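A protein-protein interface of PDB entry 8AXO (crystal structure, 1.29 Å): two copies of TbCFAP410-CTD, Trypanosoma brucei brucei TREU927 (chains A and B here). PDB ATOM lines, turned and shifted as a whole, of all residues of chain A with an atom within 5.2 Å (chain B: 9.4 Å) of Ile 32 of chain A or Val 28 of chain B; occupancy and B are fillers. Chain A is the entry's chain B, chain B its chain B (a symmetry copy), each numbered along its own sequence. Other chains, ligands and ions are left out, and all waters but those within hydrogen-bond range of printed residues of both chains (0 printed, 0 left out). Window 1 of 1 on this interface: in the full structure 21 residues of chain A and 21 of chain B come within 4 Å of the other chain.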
ATOM      1  N   VAL A  10      -4.675  15.130  23.831  1.00  0.00           N
ATOM      2  CA  VAL A  10      -3.335  15.685  23.654  1.00  0.00           C
ATOM      3  C   VAL A  10      -2.908  16.452  24.898  1.00  0.00           C
ATOM      4  O   VAL A  10      -1.771  16.320  25.366  1.00  0.00           O
ATOM      5  CB  VAL A  10      -3.269  16.548  22.379  1.00  0.00           C
ATOM      6  CG1 VAL A  10      -1.995  17.386  22.371  1.00  0.00           C
ATOM      7  CG2 VAL A  10      -3.351  15.660  21.139  1.00  0.00           C
ATOM      8  N   VAL A  13      -1.956  14.003  27.594  1.00  0.00           N
ATOM      9  CA  VAL A  13      -0.681  13.371  27.274  1.00  0.00           C
ATOM     10  C   VAL A  13       0.474  14.314  27.595  1.00  0.00           C
ATOM     11  O   VAL A  13       1.500  13.900  28.144  1.00  0.00           O
ATOM     12  CB  VAL A  13      -0.679  12.915  25.804  1.00  0.00           C
ATOM     13  CG1 VAL A  13       0.728  12.556  25.364  1.00  0.00           C
ATOM     14  CG2 VAL A  13      -1.614  11.731  25.615  1.00  0.00           C
ATOM     15  N   LEU A  17       3.605  13.433  29.991  1.00  0.00           N
ATOM     16  CA  LEU A  17       4.961  13.372  29.471  1.00  0.00           C
ATOM     17  C   LEU A  17       5.889  14.335  30.193  1.00  0.00           C
ATOM     18  O   LEU A  17       7.083  14.051  30.335  1.00  0.00           O
ATOM     19  CB  LEU A  17       4.956  13.704  27.987  1.00  0.00           C
ATOM     20  CG  LEU A  17       4.260  12.735  27.038  1.00  0.00           C
ATOM     21  CD1 LEU A  17       4.146  13.374  25.654  1.00  0.00           C
ATOM     22  CD2 LEU A  17       4.995  11.422  26.968  1.00  0.00           C
ATOM     23  N   VAL A  28       8.416   6.551  24.437  1.00  0.00           N
ATOM     24  CA  VAL A  28       7.196   7.093  23.845  1.00  0.00           C
ATOM     25  C   VAL A  28       7.454   7.561  22.415  1.00  0.00           C
ATOM     26  O   VAL A  28       6.622   7.365  21.517  1.00  0.00           O
ATOM     27  CB  VAL A  28       6.619   8.211  24.735  1.00  0.00           C
ATOM     28  CG1 VAL A  28       5.499   8.931  23.993  1.00  0.00           C
ATOM     29  CG2 VAL A  28       6.129   7.646  26.059  1.00  0.00           C
ATOM     30  N   ARG A  29       8.602   8.193  22.175  1.00  0.00           N
ATOM     31  CA  ARG A  29       8.888   8.684  20.834  1.00  0.00           C
ATOM     32  C   ARG A  29       8.979   7.539  19.832  1.00  0.00           C
ATOM     33  O   ARG A  29       8.465   7.636  18.711  1.00  0.00           O
ATOM     34  CB  ARG A  29      10.171   9.503  20.830  1.00  0.00           C
ATOM     35  CG  ARG A  29      10.291  10.373  19.598  1.00  0.00           C
ATOM     36  CD  ARG A  29      11.722  10.825  19.379  1.00  0.00           C
ATOM     37  NE  ARG A  29      12.121  11.846  20.337  1.00  0.00           N
ATOM     38  CZ  ARG A  29      13.010  11.655  21.307  1.00  0.00           C
ATOM     39  NH1 ARG A  29      13.600  10.474  21.452  1.00  0.00           N
ATOM     40  NH2 ARG A  29      13.319  12.651  22.122  1.00  0.00           N
ATOM     41  N   ARG A  30       9.658   6.457  20.204  1.00  0.00           N
ATOM     42  CA  ARG A  30       9.721   5.306  19.310  1.00  0.00           C
ATOM     43  C   ARG A  30       8.322   4.807  18.979  1.00  0.00           C
ATOM     44  O   ARG A  30       8.044   4.411  17.841  1.00  0.00           O
ATOM     45  CB  ARG A  30      10.553   4.193  19.946  1.00  0.00           C
ATOM     46  CG  ARG A  30      12.038   4.523  20.079  1.00  0.00           C
ATOM     47  CD  ARG A  30      12.863   3.298  20.442  1.00  0.00           C
ATOM     48  NE  ARG A  30      12.693   2.878  21.832  1.00  0.00           N
ATOM     49  CZ  ARG A  30      13.444   3.306  22.843  1.00  0.00           C
ATOM     50  NH1 ARG A  30      14.418   4.177  22.627  1.00  0.00           N
ATOM     51  NH2 ARG A  30      13.220   2.864  24.072  1.00  0.00           N
ATOM     52  N   PHE A  31       7.432   4.814  19.971  1.00  0.00           N
ATOM     53  CA  PHE A  31       6.064   4.365  19.749  1.00  0.00           C
ATOM     54  C   PHE A  31       5.334   5.293  18.790  1.00  0.00           C
ATOM     55  O   PHE A  31       4.651   4.823  17.874  1.00  0.00           O
ATOM     56  CB  PHE A  31       5.343   4.280  21.095  1.00  0.00           C
ATOM     57  CG  PHE A  31       3.969   3.703  21.018  1.00  0.00           C
ATOM     58  CD1 PHE A  31       3.779   2.338  20.963  1.00  0.00           C
ATOM     59  CD2 PHE A  31       2.861   4.528  21.024  1.00  0.00           C
ATOM     60  CE1 PHE A  31       2.508   1.804  20.899  1.00  0.00           C
ATOM     61  CE2 PHE A  31       1.588   4.003  20.955  1.00  0.00           C
ATOM     62  CZ  PHE A  31       1.414   2.636  20.894  1.00  0.00           C
ATOM     63  N   ILE A  32       5.486   6.608  18.962  1.00  0.00           N
ATOM     64  CA  ILE A  32       4.838   7.543  18.043  1.00  0.00           C
ATOM     65  C   ILE A  32       5.309   7.319  16.614  1.00  0.00           C
ATOM     66  O   ILE A  32       4.512   7.347  15.668  1.00  0.00           O
ATOM     67  CB  ILE A  32       5.088   8.992  18.488  1.00  0.00           C
ATOM     68  CG1 ILE A  32       4.348   9.309  19.772  1.00  0.00           C
ATOM     69  CG2 ILE A  32       4.670   9.967  17.383  1.00  0.00           C
ATOM     70  CD1 ILE A  32       4.672  10.661  20.322  1.00  0.00           C
ATOM     71  N   ASP A  33       6.608   7.094  16.429  1.00  0.00           N
ATOM     72  CA  ASP A  33       7.151   6.838  15.095  1.00  0.00           C
ATOM     73  C   ASP A  33       6.600   5.556  14.483  1.00  0.00           C
ATOM     74  O   ASP A  33       6.631   5.407  13.258  1.00  0.00           O
ATOM     75  CB  ASP A  33       8.675   6.981  15.134  1.00  0.00           C
ATOM     76  CG  ASP A  33       9.102   8.444  15.358  1.00  0.00           C
ATOM     77  OD1 ASP A  33       8.265   9.358  15.162  1.00  0.00           O
ATOM     78  OD2 ASP A  33      10.259   8.699  15.743  1.00  0.00           O
ATOM     79  N   ALA A  34       6.106   4.629  15.303  1.00  0.00           N
ATOM     80  CA  ALA A  34       5.447   3.440  14.780  1.00  0.00           C
ATOM     81  C   ALA A  34       4.026   3.724  14.307  1.00  0.00           C
ATOM     82  O   ALA A  34       3.478   2.945  13.522  1.00  0.00           O
ATOM     83  CB  ALA A  34       5.407   2.350  15.847  1.00  0.00           C
ATOM     84  N   LEU A  35       3.418   4.814  14.771  1.00  0.00           N
ATOM     85  CA  LEU A  35       2.034   5.129  14.454  1.00  0.00           C
ATOM     86  C   LEU A  35       1.880   5.918  13.161  1.00  0.00           C
ATOM     87  O   LEU A  35       0.746   6.165  12.737  1.00  0.00           O
ATOM     88  CB  LEU A  35       1.408   5.921  15.611  1.00  0.00           C
ATOM     89  CG  LEU A  35       1.358   5.230  16.974  1.00  0.00           C
ATOM     90  CD1 LEU A  35       0.857   6.169  18.062  1.00  0.00           C
ATOM     91  CD2 LEU A  35       0.488   3.980  16.889  1.00  0.00           C
ATOM     92  N   GLN A  36       2.978   6.294  12.518  1.00  0.00           N
ATOM     93  CA  GLN A  36       2.920   7.046  11.273  1.00  0.00           C
ATOM     94  C   GLN A  36       3.840   6.403  10.237  1.00  0.00           C
ATOM     95  O   GLN A  36       4.758   5.653  10.587  1.00  0.00           O
ATOM     96  CB  GLN A  36       3.341   8.494  11.508  1.00  0.00           C
ATOM     97  CG  GLN A  36       2.595   9.178  12.632  1.00  0.00           C
ATOM     98  CD  GLN A  36       3.405  10.295  13.274  1.00  0.00           C
ATOM     99  OE1 GLN A  36       4.375  10.044  13.995  1.00  0.00           O
ATOM    100  NE2 GLN A  36       3.017  11.540  13.003  1.00  0.00           N
ATOM    101  OXT GLN A  36       3.704   6.625   9.031  1.00  0.00           O
ATOM    102  N   VAL B  13       0.146   6.274  28.247  1.00  0.00           N
ATOM    103  CA  VAL B  13       0.390   7.198  27.147  1.00  0.00           C
ATOM    104  C   VAL B  13       0.320   6.465  25.812  1.00  0.00           C
ATOM    105  O   VAL B  13      -0.253   6.966  24.838  1.00  0.00           O
ATOM    106  CB  VAL B  13       1.736   7.915  27.357  1.00  0.00           C
ATOM    107  CG1 VAL B  13       2.160   8.626  26.084  1.00  0.00           C
ATOM    108  CG2 VAL B  13       1.639   8.900  28.509  1.00  0.00           C
ATOM    109  N   LYS B  14       0.881   5.260  25.750  1.00  0.00           N
ATOM    110  CA  LYS B  14       0.831   4.502  24.503  1.00  0.00           C
ATOM    111  C   LYS B  14      -0.605   4.202  24.092  1.00  0.00           C
ATOM    112  O   LYS B  14      -0.961   4.321  22.914  1.00  0.00           O
ATOM    113  CB  LYS B  14       1.601   3.199  24.663  1.00  0.00           C
ATOM    114  CG  LYS B  14       3.097   3.362  24.678  1.00  0.00           C
ATOM    115  CD  LYS B  14       3.775   2.011  24.796  1.00  0.00           C
ATOM    116  CE  LYS B  14       5.274   2.161  24.844  1.00  0.00           C
ATOM    117  NZ  LYS B  14       5.932   0.842  25.024  1.00  0.00           N
ATOM    118  N   LEU B  16      -3.254   5.970  24.777  1.00  0.00           N
ATOM    119  CA  LEU B  16      -3.872   7.205  24.304  1.00  0.00           C
ATOM    120  C   LEU B  16      -3.361   7.595  22.925  1.00  0.00           C
ATOM    121  O   LEU B  16      -4.143   7.988  22.050  1.00  0.00           O
ATOM    122  CB  LEU B  16      -3.610   8.332  25.296  1.00  0.00           C
ATOM    123  CG  LEU B  16      -4.279   8.155  26.652  1.00  0.00           C
ATOM    124  CD1 LEU B  16      -3.744   9.219  27.607  1.00  0.00           C
ATOM    125  CD2 LEU B  16      -5.780   8.256  26.546  1.00  0.00           C
ATOM    126  N   LEU B  17      -2.057   7.492  22.710  1.00  0.00           N
ATOM    127  CA  LEU B  17      -1.497   7.921  21.439  1.00  0.00           C
ATOM    128  C   LEU B  17      -1.965   7.047  20.288  1.00  0.00           C
ATOM    129  O   LEU B  17      -2.107   7.535  19.161  1.00  0.00           O
ATOM    130  CB  LEU B  17       0.022   7.882  21.508  1.00  0.00           C
ATOM    131  CG  LEU B  17       0.722   8.851  22.453  1.00  0.00           C
ATOM    132  CD1 LEU B  17       2.200   8.475  22.561  1.00  0.00           C
ATOM    133  CD2 LEU B  17       0.559  10.274  21.988  1.00  0.00           C
ATOM    134  N   SER B  18      -2.206   5.760  20.549  1.00  0.00           N
ATOM    135  CA  SER B  18      -2.453   4.807  19.475  1.00  0.00           C
ATOM    136  C   SER B  18      -3.699   5.146  18.680  1.00  0.00           C
ATOM    137  O   SER B  18      -3.848   4.661  17.552  1.00  0.00           O
ATOM    138  CB  SER B  18      -2.560   3.405  20.065  1.00  0.00           C
ATOM    139  OG  SER B  18      -3.763   3.276  20.793  1.00  0.00           O
ATOM    140  N   LEU B  20      -4.726   8.439  18.008  1.00  0.00           N
ATOM    141  CA  LEU B  20      -4.752   9.832  17.596  1.00  0.00           C
ATOM    142  C   LEU B  20      -4.463   9.988  16.106  1.00  0.00           C
ATOM    143  O   LEU B  20      -3.832   9.139  15.468  1.00  0.00           O
ATOM    144  CB  LEU B  20      -3.707  10.634  18.367  1.00  0.00           C
ATOM    145  CG  LEU B  20      -3.842  10.746  19.882  1.00  0.00           C
ATOM    146  CD1 LEU B  20      -2.792  11.729  20.409  1.00  0.00           C
ATOM    147  CD2 LEU B  20      -5.234  11.172  20.283  1.00  0.00           C
ATOM    148  N   SER B  21      -4.919  11.115  15.560  1.00  0.00           N
ATOM    149  CA  SER B  21      -4.618  11.471  14.187  1.00  0.00           C
ATOM    150  C   SER B  21      -3.177  11.962  14.065  1.00  0.00           C
ATOM    151  O   SER B  21      -2.485  12.206  15.060  1.00  0.00           O
ATOM    152  CB  SER B  21      -5.554  12.581  13.715  1.00  0.00           C
ATOM    153  OG  SER B  21      -5.157  13.832  14.254  1.00  0.00           O
ATOM    154  N   VAL B  22      -2.721  12.093  12.816  1.00  0.00           N
ATOM    155  CA  VAL B  22      -1.369  12.585  12.574  1.00  0.00           C
ATOM    156  C   VAL B  22      -1.198  13.976  13.172  1.00  0.00           C
ATOM    157  O   VAL B  22      -0.128  14.314  13.684  1.00  0.00           O
ATOM    158  CB  VAL B  22      -1.040  12.560  11.072  1.00  0.00           C
ATOM    159  CG1 VAL B  22      -0.791  11.126  10.620  1.00  0.00           C
ATOM    160  CG2 VAL B  22      -2.162  13.192  10.271  1.00  0.00           C
ATOM    161  N   GLU B  23      -2.255  14.789  13.117  1.00  0.00           N
ATOM    162  CA  GLU B  23      -2.194  16.129  13.694  1.00  0.00           C
ATOM    163  C   GLU B  23      -1.846  16.063  15.174  1.00  0.00           C
ATOM    164  O   GLU B  23      -0.934  16.754  15.641  1.00  0.00           O
ATOM    165  CB  GLU B  23      -3.538  16.837  13.489  1.00  0.00           C
ATOM    166  CG  GLU B  23      -3.598  18.258  14.013  1.00  0.00           C
ATOM    167  CD  GLU B  23      -4.314  19.205  13.056  1.00  0.00           C
ATOM    168  OE1 GLU B  23      -4.753  18.762  11.968  1.00  0.00           O
ATOM    169  OE2 GLU B  23      -4.427  20.405  13.390  1.00  0.00           O
ATOM    170  N   GLY B  24      -2.564  15.226  15.922  1.00  0.00           N
ATOM    171  CA  GLY B  24      -2.295  15.103  17.343  1.00  0.00           C
ATOM    172  C   GLY B  24      -0.942  14.488  17.630  1.00  0.00           C
ATOM    173  O   GLY B  24      -0.230  14.937  18.531  1.00  0.00           O
ATOM    174  N   LEU B  25      -0.567  13.461  16.868  1.00  0.00           N
ATOM    175  CA  LEU B  25       0.737  12.839  17.066  1.00  0.00           C
ATOM    176  C   LEU B  25       1.862  13.832  16.802  1.00  0.00           C
ATOM    177  O   LEU B  25       2.861  13.863  17.532  1.00  0.00           O
ATOM    178  CB  LEU B  25       0.872  11.616  16.163  1.00  0.00           C
ATOM    179  CG  LEU B  25      -0.052  10.442  16.480  1.00  0.00           C
ATOM    180  CD1 LEU B  25       0.075   9.381  15.397  1.00  0.00           C
ATOM    181  CD2 LEU B  25       0.257   9.870  17.848  1.00  0.00           C
ATOM    182  N   ASP B  26       1.713  14.657  15.762  1.00  0.00           N
ATOM    183  CA  ASP B  26       2.736  15.652  15.456  1.00  0.00           C
ATOM    184  C   ASP B  26       2.862  16.671  16.581  1.00  0.00           C
ATOM    185  O   ASP B  26       3.973  17.083  16.934  1.00  0.00           O
ATOM    186  CB  ASP B  26       2.411  16.347  14.133  1.00  0.00           C
ATOM    187  CG  ASP B  26       2.642  15.449  12.933  1.00  0.00           C
ATOM    188  OD1 ASP B  26       3.294  14.396  13.097  1.00  0.00           O
ATOM    189  OD2 ASP B  26       2.173  15.796  11.827  1.00  0.00           O
ATOM    190  N   GLU B  27       1.737  17.082  17.166  1.00  0.00           N
ATOM    191  CA  GLU B  27       1.801  18.015  18.286  1.00  0.00           C
ATOM    192  C   GLU B  27       2.509  17.389  19.480  1.00  0.00           C
ATOM    193  O   GLU B  27       3.328  18.036  20.139  1.00  0.00           O
ATOM    194  CB  GLU B  27       0.395  18.470  18.672  1.00  0.00           C
ATOM    195  CG  GLU B  27       0.384  19.629  19.654  1.00  0.00           C
ATOM    196  CD  GLU B  27      -1.020  20.119  19.965  1.00  0.00           C
ATOM    197  OE1 GLU B  27      -1.938  19.852  19.154  1.00  0.00           O
ATOM    198  OE2 GLU B  27      -1.202  20.770  21.020  1.00  0.00           O
ATOM    199  N   VAL B  28       2.212  16.125  19.775  1.00  0.00           N
ATOM    200  CA  VAL B  28       2.843  15.469  20.918  1.00  0.00           C
ATOM    201  C   VAL B  28       4.350  15.342  20.699  1.00  0.00           C
ATOM    202  O   VAL B  28       5.148  15.531  21.626  1.00  0.00           O
ATOM    203  CB  VAL B  28       2.171  14.110  21.195  1.00  0.00           C
ATOM    204  CG1 VAL B  28       2.990  13.332  22.218  1.00  0.00           C
ATOM    205  CG2 VAL B  28       0.739  14.305  21.669  1.00  0.00           C
ATOM    206  N   ARG B  29       4.764  15.011  19.477  1.00  0.00           N
ATOM    207  CA  ARG B  29       6.190  14.850  19.219  1.00  0.00           C
ATOM    208  C   ARG B  29       6.943  16.157  19.432  1.00  0.00           C
ATOM    209  O   ARG B  29       8.035  16.172  20.012  1.00  0.00           O
ATOM    210  CB  ARG B  29       6.417  14.322  17.809  1.00  0.00           C
ATOM    211  CG  ARG B  29       7.804  13.743  17.633  1.00  0.00           C
ATOM    212  CD  ARG B  29       8.176  13.639  16.166  1.00  0.00           C
ATOM    213  NE  ARG B  29       7.463  12.557  15.501  1.00  0.00           N
ATOM    214  CZ  ARG B  29       6.517  12.737  14.585  1.00  0.00           C
ATOM    215  NH1 ARG B  29       6.163  13.964  14.219  1.00  0.00           N
ATOM    216  NH2 ARG B  29       5.935  11.689  14.025  1.00  0.00           N
ATOM    217  N   ARG B  30       6.391  17.264  18.940  1.00  0.00           N
ATOM    218  CA  ARG B  30       7.036  18.552  19.171  1.00  0.00           C
ATOM    219  C   ARG B  30       7.194  18.811  20.662  1.00  0.00           C
ATOM    220  O   ARG B  30       8.215  19.350  21.107  1.00  0.00           O
ATOM    221  CB  ARG B  30       6.228  19.669  18.513  1.00  0.00           C
ATOM    222  CG  ARG B  30       6.233  19.627  16.986  1.00  0.00           C
ATOM    223  CD  ARG B  30       5.670  20.902  16.379  1.00  0.00           C
ATOM    224  NE  ARG B  30       4.217  21.009  16.507  1.00  0.00           N
ATOM    225  CZ  ARG B  30       3.349  20.559  15.605  1.00  0.00           C
ATOM    226  NH1 ARG B  30       3.782  19.959  14.506  1.00  0.00           N
ATOM    227  NH2 ARG B  30       2.047  20.707  15.803  1.00  0.00           N
ATOM    228  N   PHE B  31       6.185  18.438  21.447  1.00  0.00           N
ATOM    229  CA  PHE B  31       6.248  18.635  22.889  1.00  0.00           C
ATOM    230  C   PHE B  31       7.339  17.777  23.511  1.00  0.00           C
ATOM    231  O   PHE B  31       8.108  18.263  24.346  1.00  0.00           O
ATOM    232  CB  PHE B  31       4.880  18.318  23.495  1.00  0.00           C
ATOM    233  CG  PHE B  31       4.775  18.609  24.956  1.00  0.00           C
ATOM    234  CD1 PHE B  31       4.545  19.893  25.402  1.00  0.00           C
ATOM    235  CD2 PHE B  31       4.885  17.591  25.884  1.00  0.00           C
ATOM    236  CE1 PHE B  31       4.440  20.162  26.754  1.00  0.00           C
ATOM    237  CE2 PHE B  31       4.786  17.853  27.233  1.00  0.00           C
ATOM    238  CZ  PHE B  31       4.562  19.142  27.668  1.00  0.00           C
ATOM    239  N   ILE B  32       7.443  16.511  23.099  1.00  0.00           N
ATOM    240  CA  ILE B  32       8.501  15.655  23.634  1.00  0.00           C
ATOM    241  C   ILE B  32       9.876  16.236  23.338  1.00  0.00           C
ATOM    242  O   ILE B  32      10.769  16.227  24.192  1.00  0.00           O
ATOM    243  CB  ILE B  32       8.370  14.229  23.079  1.00  0.00           C
ATOM    244  CG1 ILE B  32       7.143  13.533  23.633  1.00  0.00           C
ATOM    245  CG2 ILE B  32       9.629  13.416  23.397  1.00  0.00           C
ATOM    246  CD1 ILE B  32       6.893  12.196  23.014  1.00  0.00           C
ATOM    247  N   ASP B  33      10.072  16.749  22.125  1.00  0.00           N
ATOM    248  CA  ASP B  33      11.350  17.356  21.756  1.00  0.00           C
ATOM    249  C   ASP B  33      11.664  18.593  22.589  1.00  0.00           C
ATOM    250  O   ASP B  33      12.834  18.973  22.693  1.00  0.00           O
ATOM    251  CB  ASP B  33      11.411  17.520  20.235  1.00  0.00           C
ATOM    252  CG  ASP B  33      11.507  16.157  19.522  1.00  0.00           C
ATOM    253  OD1 ASP B  33      11.844  15.146  20.185  1.00  0.00           O
ATOM    254  OD2 ASP B  33      11.236  16.072  18.309  1.00  0.00           O
ATOM    255  N   ALA B  34      10.652  19.229  23.178  1.00  0.00           N
ATOM    256  CA  ALA B  34      10.893  20.338  24.092  1.00  0.00           C
ATOM    257  C   ALA B  34      11.347  19.867  25.468  1.00  0.00           C
ATOM    258  O   ALA B  34      11.933  20.653  26.218  1.00  0.00           O
ATOM    259  CB  ALA B  34       9.627  21.176  24.245  1.00  0.00           C
ATOM    260  N   LEU B  35      11.084  18.609  25.818  1.00  0.00           N
ATOM    261  CA  LEU B  35      11.395  18.087  27.140  1.00  0.00           C
ATOM    262  C   LEU B  35      12.812  17.542  27.252  1.00  0.00           C
ATOM    263  O   LEU B  35      13.225  17.155  28.350  1.00  0.00           O
ATOM    264  CB  LEU B  35      10.395  16.981  27.504  1.00  0.00           C
ATOM    265  CG  LEU B  35       8.919  17.378  27.566  1.00  0.00           C
ATOM    266  CD1 LEU B  35       8.020  16.169  27.787  1.00  0.00           C
ATOM    267  CD2 LEU B  35       8.709  18.420  28.660  1.00  0.00           C
ATOM    268  N   GLN B  36      13.568  17.523  26.161  1.00  0.00           N
ATOM    269  CA  GLN B  36      14.935  17.024  26.182  1.00  0.00           C
ATOM    270  C   GLN B  36      15.861  18.023  25.491  1.00  0.00           C
ATOM    271  O   GLN B  36      15.410  18.862  24.705  1.00  0.00           O
ATOM    272  CB  GLN B  36      15.017  15.673  25.477  1.00  0.00           C
ATOM    273  CG  GLN B  36      14.021  14.653  25.982  1.00  0.00           C
ATOM    274  CD  GLN B  36      13.655  13.621  24.923  1.00  0.00           C
ATOM    275  OE1 GLN B  36      12.944  13.922  23.962  1.00  0.00           O
ATOM    276  NE2 GLN B  36      14.154  12.397  25.092  1.00  0.00           N
ATOM    277  OXT GLN B  36      17.079  18.010  25.685  1.00  0.00           O
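The guanidinium group (NE) of Arg 29 of chain A lies within salt-bridge range of the side-chain carboxylate (OD1) of Asp 33 of chain B, at 3.3 Å. The side-chain amide nitrogen of Gln 36 of chain B sits close to the guanidinium group of Arg 29 of chain A. The side-chain carboxylate (OD1) of Asp 33 of chain A is in salt-bridge range of the guanidinium group (NE) of Arg 29 of chain B (3.3 Å). The side-chain amide nitrogen (NE2) of Gln 36 of chain A sits at hydrogen-bond distance from the side-chain carboxylate (OD1) of Asp 26 of chain B, at 2.9 Å. The side-chain amide nitrogen (NE2) of Gln 36 of chain A sits close to the guanidinium group (NH2) of Arg 29 of chain B.
The side-chain amide oxygen (OE1) of Gln 36 of chain A lies close to the backbone carbonyl oxygen (O) of Ile 32 of chain A. The side-chain hydroxyl of Ser 21 of chain B lies within hydrogen-bond range of the backbone NH of Gly 24 of chain B, at 3.4 Å. The side-chain carboxylate (OD1) of Asp 26 of chain B is in salt-bridge range of the guanidinium group (NH1) of Arg 29 of chain B (3.1 Å). The backbone carbonyl oxygen (O) of Ile 32 of chain B lies close to the side-chain amide oxygen (OE1) of Gln 36 of chain B (3.2 Å).
Among the printed residues, pairs that only touch across the chains: Phe 31 of chain A with Lys 14 of chain B (3.2 Å), Leu 17 of chain A with Leu 35 of chain B (3.4 Å), Leu 35 of chain A with Leu 17 of chain B (3.4 Å), Ile 32 of chain A with Leu 17 of chain B (3.6 Å), Leu 17 of chain A with Ile 32 of chain B (3.6 Å), Val 28 of chain A with Leu 17 of chain B (3.6 Å), Leu 17 of chain A with Val 28 of chain B (3.6 Å), Ile 32 of chain A with Val 28 of chain B (3.7 Å), Val 28 of chain A with Ile 32 of chain B (3.7 Å), Leu 35 of chain A with Leu 25 of chain B (3.7 Å), Val 10 of chain A with Glu 27 of chain B (3.7 Å), Gln 36 of chain A with Leu 25 of chain B (3.7 Å), Ile 32 of chain A with Ile 32 of chain B (3.8 Å), Leu 35 of chain A with Ser 18 of chain B (3.8 Å), Val 13 of chain A with Leu 16 of chain B (3.8 Å), Val 28 of chain A with Val 13 of chain B (3.95 Å), Val 13 of chain A with Val 28 of chain B (3.95 Å), Arg 29 of chain A with Ile 32 of chain B (3.98 Å), Val 10 of chain A with Gly 24 of chain B (3.98 Å) and Ile 32 of chain A with Arg 29 of chain B (3.98 Å).
Of the printed residues of chain B, Ile 32 of chain A touches Leu 17, Val 28, Arg 29 and Ile 32. Val 28 of chain B touches just these residues of chain A: Val 13 (3.95 Å), Leu 17 (3.6 Å) and Ile 32 (3.7 Å). Asp 33 of chain A touches just one residue of chain B: Arg 29. Of the printed residues of chain A, Ser 18 of chain B touches Leu 35 (3.8 Å). Printed residues of chain B within 4 Å of Leu 35 of chain A: Leu 17, Ser 18 and Leu 25. Ala 34 of chain B touches none of the printed residues of chain A. The nearest residue of chain A that does not touch Val 28 of chain B is Val 10 of chain A (4.2 Å). The nearest printed residue of chain B that does not touch Val 28 of chain A is Val 28 of chain B (5.4 Å).
Of the 12 printed residues of chain A, 10 touch a printed residue of chain B. Hydrophobic or aromatic side chains of chain B within 4 Å of the printed part of chain A: Val 13, Leu 16, Leu 17, Leu 25, Val 28, Ile 32 and Leu 35. Among the printed residues, 25 pairs touch across the chains.
Leu 17 of chain A touches Leu 35 of chain B, and with the chains exchanged Leu 35 of chain A touches Leu 17 of chain B. Val 28 of chain A touches Ile 32 of chain B, and with the chains exchanged Ile 32 of chain A touches Val 28 of chain B. Arg 29 of chain A touches Gln 36 of chain B, and with the chains exchanged Gln 36 of chain A touches Arg 29 of chain B. Ile 32 of chain B touches its own counterpart, Ile 32 of chain A. Positions printed for both chains: 13, 17, 28, 29, 30, 31, 32, 33, 34, 35 and 36.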
